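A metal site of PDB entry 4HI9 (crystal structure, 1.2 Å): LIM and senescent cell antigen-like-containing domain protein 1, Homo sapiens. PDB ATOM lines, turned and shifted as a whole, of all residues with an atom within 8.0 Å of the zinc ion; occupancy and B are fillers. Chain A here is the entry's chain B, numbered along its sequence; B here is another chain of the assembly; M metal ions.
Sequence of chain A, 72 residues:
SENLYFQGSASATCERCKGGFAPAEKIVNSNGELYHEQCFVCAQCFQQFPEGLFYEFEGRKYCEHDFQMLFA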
ATOM      1  N   THR A  13      21.739  -9.478   4.655  1.00  0.00           N
ATOM      2  CA  THR A  13      20.420  -8.889   4.854  1.00  0.00           C
ATOM      3  C   THR A  13      19.319  -9.914   4.617  1.00  0.00           C
ATOM      4  O   THR A  13      19.499 -10.887   3.862  1.00  0.00           O
ATOM      5  CB  THR A  13      20.186  -7.663   3.887  1.00  0.00           C
ATOM      6  OG1 THR A  13      20.241  -8.090   2.528  1.00  0.00           O
ATOM      7  CG2 THR A  13      21.220  -6.582   4.094  1.00  0.00           C
ATOM      8  N   CYS A  14      18.182  -9.726   5.298  1.00  0.00           N
ATOM      9  CA  CYS A  14      16.991 -10.562   5.120  1.00  0.00           C
ATOM     10  C   CYS A  14      16.394 -10.313   3.732  1.00  0.00           C
ATOM     11  O   CYS A  14      16.156  -9.172   3.336  1.00  0.00           O
ATOM     12  CB  CYS A  14      15.972 -10.253   6.227  1.00  0.00           C
ATOM     13  SG  CYS A  14      14.372 -11.107   6.111  1.00  0.00           S
ATOM     14  N   GLU A  15      16.113 -11.389   3.016  1.00  0.00           N
ATOM     15  CA  GLU A  15      15.523 -11.296   1.676  1.00  0.00           C
ATOM     16  C   GLU A  15      14.153 -10.581   1.690  1.00  0.00           C
ATOM     17  O   GLU A  15      13.799  -9.876   0.738  1.00  0.00           O
ATOM     18  CB  GLU A  15      15.402 -12.711   1.078  1.00  0.00           C
ATOM     19  CG  GLU A  15      14.630 -12.815  -0.247  1.00  0.00           C
ATOM     20  CD  GLU A  15      15.269 -12.062  -1.395  1.00  0.00           C
ATOM     21  OE1 GLU A  15      16.493 -11.809  -1.359  1.00  0.00           O
ATOM     22  OE2 GLU A  15      14.539 -11.711  -2.347  1.00  0.00           O
ATOM     23  N   ARG A  16      13.374 -10.723   2.775  1.00  0.00           N
ATOM     24  CA  ARG A  16      12.045 -10.130   2.827  1.00  0.00           C
ATOM     25  C   ARG A  16      12.090  -8.686   3.252  1.00  0.00           C
ATOM     26  O   ARG A  16      11.598  -7.852   2.517  1.00  0.00           O
ATOM     27  CB  ARG A  16      11.104 -10.898   3.748  1.00  0.00           C
ATOM     28  CG  ARG A  16       9.663 -10.451   3.596  1.00  0.00           C
ATOM     29  CD  ARG A  16       8.778 -10.938   4.732  1.00  0.00           C
ATOM     30  NE  ARG A  16       8.935 -10.172   5.972  1.00  0.00           N
ATOM     31  CZ  ARG A  16       8.321  -9.021   6.206  1.00  0.00           C
ATOM     32  NH1 ARG A  16       7.631  -8.437   5.224  1.00  0.00           N
ATOM     33  NH2 ARG A  16       8.500  -8.413   7.375  1.00  0.00           N
ATOM     34  N   CYS A  17      12.653  -8.398   4.434  1.00  0.00           N
ATOM     35  CA  CYS A  17      12.518  -7.086   5.084  1.00  0.00           C
ATOM     36  C   CYS A  17      13.762  -6.213   4.961  1.00  0.00           C
ATOM     37  O   CYS A  17      13.718  -5.033   5.315  1.00  0.00           O
ATOM     38  CB  CYS A  17      12.172  -7.259   6.570  1.00  0.00           C
ATOM     39  SG  CYS A  17      13.564  -7.678   7.663  1.00  0.00           S
ATOM     40  N   LYS A  18      14.848  -6.809   4.473  1.00  0.00           N
ATOM     41  CA  LYS A  18      16.105  -6.105   4.186  1.00  0.00           C
ATOM     42  C   LYS A  18      16.897  -5.671   5.431  1.00  0.00           C
ATOM     43  O   LYS A  18      17.912  -4.982   5.318  1.00  0.00           O
ATOM     44  CB  LYS A  18      15.865  -4.906   3.251  1.00  0.00           C
ATOM     45  CG  LYS A  18      15.135  -5.251   1.955  1.00  0.00           C
ATOM     46  CD  LYS A  18      16.087  -5.484   0.781  1.00  0.00           C
ATOM     47  CE  LYS A  18      15.328  -5.668  -0.542  1.00  0.00           C
ATOM     48  NZ  LYS A  18      14.404  -6.843  -0.529  1.00  0.00           N
ATOM     49  N   GLY A  19      16.444  -6.091   6.611  1.00  0.00           N
ATOM     50  CA  GLY A  19      17.183  -5.825   7.836  1.00  0.00           C
ATOM     51  C   GLY A  19      18.311  -6.821   8.080  1.00  0.00           C
ATOM     52  O   GLY A  19      18.353  -7.902   7.496  1.00  0.00           O
ATOM     53  N   GLY A  20      19.243  -6.443   8.947  1.00  0.00           N
ATOM     54  CA  GLY A  20      20.381  -7.301   9.228  1.00  0.00           C
ATOM     55  C   GLY A  20      20.138  -8.291  10.345  1.00  0.00           C
ATOM     56  O   GLY A  20      19.047  -8.327  10.940  1.00  0.00           O
ATOM     57  N   PHE A  21      21.161  -9.102  10.625  1.00  0.00           N
ATOM     58  CA  PHE A  21      21.092 -10.168  11.631  1.00  0.00           C
ATOM     59  C   PHE A  21      22.063  -9.935  12.787  1.00  0.00           C
ATOM     60  O   PHE A  21      23.134  -9.336  12.607  1.00  0.00           O
ATOM     61  CB  PHE A  21      21.440 -11.508  10.984  1.00  0.00           C
ATOM     62  CG  PHE A  21      20.585 -11.835   9.782  1.00  0.00           C
ATOM     63  CD1 PHE A  21      19.253 -12.136   9.941  1.00  0.00           C
ATOM     64  CD2 PHE A  21      21.137 -11.869   8.511  1.00  0.00           C
ATOM     65  CE1 PHE A  21      18.447 -12.430   8.839  1.00  0.00           C
ATOM     66  CE2 PHE A  21      20.357 -12.180   7.403  1.00  0.00           C
ATOM     67  CZ  PHE A  21      19.007 -12.468   7.563  1.00  0.00           C
ATOM     68  N   GLU A  25      21.916 -15.286  16.036  1.00  0.00           N
ATOM     69  CA  GLU A  25      20.473 -15.282  15.763  1.00  0.00           C
ATOM     70  C   GLU A  25      20.065 -16.493  14.917  1.00  0.00           C
ATOM     71  O   GLU A  25      20.730 -16.838  13.958  1.00  0.00           O
ATOM     72  CB  GLU A  25      20.055 -14.000  15.034  1.00  0.00           C
ATOM     73  CG  GLU A  25      18.560 -13.938  14.753  1.00  0.00           C
ATOM     74  CD  GLU A  25      18.088 -12.615  14.156  1.00  0.00           C
ATOM     75  OE1 GLU A  25      18.925 -11.717  13.936  1.00  0.00           O
ATOM     76  OE2 GLU A  25      16.869 -12.478  13.925  1.00  0.00           O
ATOM     77  N   LEU A  34      18.497 -15.602   2.839  1.00  0.00           N
ATOM     78  CA  LEU A  34      18.432 -15.593   4.300  1.00  0.00           C
ATOM     79  C   LEU A  34      17.263 -14.786   4.798  1.00  0.00           C
ATOM     80  O   LEU A  34      16.963 -13.720   4.249  1.00  0.00           O
ATOM     81  CB  LEU A  34      19.705 -15.010   4.905  1.00  0.00           C
ATOM     82  CG  LEU A  34      21.009 -15.658   4.427  1.00  0.00           C
ATOM     83  CD1 LEU A  34      22.203 -14.984   5.080  1.00  0.00           C
ATOM     84  CD2 LEU A  34      21.030 -17.173   4.705  1.00  0.00           C
ATOM     85  N   TYR A  35      16.606 -15.329   5.813  1.00  0.00           N
ATOM     86  CA  TYR A  35      15.424 -14.703   6.409  1.00  0.00           C
ATOM     87  C   TYR A  35      15.477 -14.714   7.940  1.00  0.00           C
ATOM     88  O   TYR A  35      15.892 -15.705   8.541  1.00  0.00           O
ATOM     89  CB  TYR A  35      14.159 -15.496   6.028  1.00  0.00           C
ATOM     90  CG  TYR A  35      13.859 -15.562   4.564  1.00  0.00           C
ATOM     91  CD1 TYR A  35      14.479 -16.492   3.759  1.00  0.00           C
ATOM     92  CD2 TYR A  35      12.965 -14.665   3.987  1.00  0.00           C
ATOM     93  CE1 TYR A  35      14.210 -16.567   2.419  1.00  0.00           C
ATOM     94  CE2 TYR A  35      12.664 -14.731   2.650  1.00  0.00           C
ATOM     95  CZ  TYR A  35      13.300 -15.693   1.855  1.00  0.00           C
ATOM     96  OH  TYR A  35      13.045 -15.764   0.515  1.00  0.00           O
ATOM     97  N   HIS A  36      14.973 -13.652   8.562  1.00  0.00           N
ATOM     98  CA  HIS A  36      14.559 -13.719   9.977  1.00  0.00           C
ATOM     99  C   HIS A  36      13.515 -14.823  10.136  1.00  0.00           C
ATOM    100  O   HIS A  36      12.736 -15.094   9.208  1.00  0.00           O
ATOM    101  CB  HIS A  36      13.987 -12.389  10.483  1.00  0.00           C
ATOM    102  CG  HIS A  36      14.945 -11.250  10.384  1.00  0.00           C
ATOM    103  ND1 HIS A  36      14.811 -10.238   9.439  1.00  0.00           N
ATOM    104  CD2 HIS A  36      16.041 -10.949  11.104  1.00  0.00           C
ATOM    105  CE1 HIS A  36      15.806  -9.386   9.589  1.00  0.00           C
ATOM    106  NE2 HIS A  36      16.566  -9.786  10.587  1.00  0.00           N
ATOM    107  N   GLU A  37      13.460 -15.456  11.290  1.00  0.00           N
ATOM    108  CA  GLU A  37      12.391 -16.444  11.526  1.00  0.00           C
ATOM    109  C   GLU A  37      11.008 -15.847  11.292  1.00  0.00           C
ATOM    110  O   GLU A  37      10.136 -16.522  10.762  1.00  0.00           O
ATOM    111  CB  GLU A  37      12.472 -17.011  12.948  1.00  0.00           C
ATOM    112  CG  GLU A  37      13.766 -17.694  13.292  1.00  0.00           C
ATOM    113  CD  GLU A  37      14.069 -17.610  14.769  1.00  0.00           C
ATOM    114  OE1 GLU A  37      14.544 -16.546  15.226  1.00  0.00           O
ATOM    115  OE2 GLU A  37      13.804 -18.601  15.486  1.00  0.00           O
ATOM    116  N   GLN A  38      10.808 -14.591  11.703  1.00  0.00           N
ATOM    117  CA  GLN A  38       9.526 -13.907  11.571  1.00  0.00           C
ATOM    118  C   GLN A  38       9.278 -13.490  10.131  1.00  0.00           C
ATOM    119  O   GLN A  38       8.201 -12.990   9.814  1.00  0.00           O
ATOM    120  CB  GLN A  38       9.457 -12.629  12.444  1.00  0.00           C
ATOM    121  CG  GLN A  38      10.268 -12.632  13.706  1.00  0.00           C
ATOM    122  CD  GLN A  38      11.739 -12.411  13.443  1.00  0.00           C
ATOM    123  OE1 GLN A  38      12.518 -13.346  13.490  1.00  0.00           O
ATOM    124  NE2 GLN A  38      12.125 -11.167  13.158  1.00  0.00           N
ATOM    125  N   CYS A  39      10.244 -13.713   9.251  1.00  0.00           N
ATOM    126  CA  CYS A  39      10.094 -13.272   7.855  1.00  0.00           C
ATOM    127  C   CYS A  39       9.935 -14.420   6.893  1.00  0.00           C
ATOM    128  O   CYS A  39       9.434 -14.200   5.775  1.00  0.00           O
ATOM    129  CB  CYS A  39      11.292 -12.423   7.436  1.00  0.00           C
ATOM    130  SG  CYS A  39      11.331 -10.806   8.290  1.00  0.00           S
ATOM    131  N   PHE A  40      10.343 -15.626   7.288  1.00  0.00           N
ATOM    132  CA  PHE A  40      10.117 -16.801   6.448  1.00  0.00           C
ATOM    133  C   PHE A  40       8.740 -17.366   6.804  1.00  0.00           C
ATOM    134  O   PHE A  40       8.597 -18.395   7.439  1.00  0.00           O
ATOM    135  CB  PHE A  40      11.237 -17.844   6.586  1.00  0.00           C
ATOM    136  CG  PHE A  40      11.147 -18.911   5.552  1.00  0.00           C
ATOM    137  CD1 PHE A  40      11.347 -18.591   4.209  1.00  0.00           C
ATOM    138  CD2 PHE A  40      10.848 -20.219   5.907  1.00  0.00           C
ATOM    139  CE1 PHE A  40      11.254 -19.578   3.233  1.00  0.00           C
ATOM    140  CE2 PHE A  40      10.775 -21.190   4.952  1.00  0.00           C
ATOM    141  CZ  PHE A  40      10.976 -20.876   3.617  1.00  0.00           C
ATOM    142  N   PHE B 114       3.603  -5.048   8.259  1.00  0.00           N
ATOM    143  CA  PHE B 114       4.433  -6.196   7.836  1.00  0.00           C
ATOM    144  C   PHE B 114       5.323  -5.795   6.672  1.00  0.00           C
ATOM    145  O   PHE B 114       6.476  -6.248   6.613  1.00  0.00           O
ATOM    146  CB  PHE B 114       3.514  -7.365   7.448  1.00  0.00           C
ATOM    147  CG  PHE B 114       4.245  -8.649   7.114  1.00  0.00           C
ATOM    148  CD1 PHE B 114       4.885  -9.377   8.104  1.00  0.00           C
ATOM    149  CD2 PHE B 114       4.202  -9.158   5.844  1.00  0.00           C
ATOM    150  CE1 PHE B 114       5.514 -10.599   7.802  1.00  0.00           C
ATOM    151  CE2 PHE B 114       4.851 -10.375   5.529  1.00  0.00           C
ATOM    152  CZ  PHE B 114       5.479 -11.082   6.524  1.00  0.00           C
ATOM    153  N   LYS B 146       8.775  -3.552  11.991  1.00  0.00           N
ATOM    154  CA  LYS B 146      10.120  -3.425  12.548  1.00  0.00           C
ATOM    155  C   LYS B 146      10.105  -2.388  13.662  1.00  0.00           C
ATOM    156  O   LYS B 146       9.213  -1.534  13.722  1.00  0.00           O
ATOM    157  CB  LYS B 146      11.097  -2.941  11.487  1.00  0.00           C
ATOM    158  CG  LYS B 146      11.339  -3.920  10.372  1.00  0.00           C
ATOM    159  CD  LYS B 146      12.296  -3.283   9.390  1.00  0.00           C
ATOM    160  CE  LYS B 146      12.803  -4.275   8.377  1.00  0.00           C
ATOM    161  NZ  LYS B 146      13.960  -3.709   7.622  1.00  0.00           N
HETATM  162 ZN    ZN M   1      13.395  -9.992   7.909  1.00  0.00          ZN
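A ring nitrogen (NE2) of His 36 is in hydrogen-bond range of the backbone carbonyl oxygen of Gly 20 (2.9 Å). The side-chain sulfur of Cys 39 sits close to the guanidinium group of Arg 16. The backbone NH (N) of Arg 16 sits close to the side-chain sulfur (SG) of Cys 14, 3.5 Å away. The backbone NH (N) of Cys 14 is in hydrogen-bond range of the backbone carbonyl oxygen (O) of Gly 19 (2.9 Å). SG of Cys 17 lies close to N of Gly 19, at 3.5 Å. NZ of Lys 146 of chain B is in hydrogen-bond range of O of Cys 17, at 2.7 Å.
Of the 19 residues printed, 4 come within 4 Å of the zinc ion.
The zinc ion is bound by ND1 of His 36 (2.1 Å), SG of Cys 39 (2.3 Å), SG of Cys 14 (2.3 Å) and SG of Cys 17 (2.3 Å). The zinc ion has four donor atoms within binding distance.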
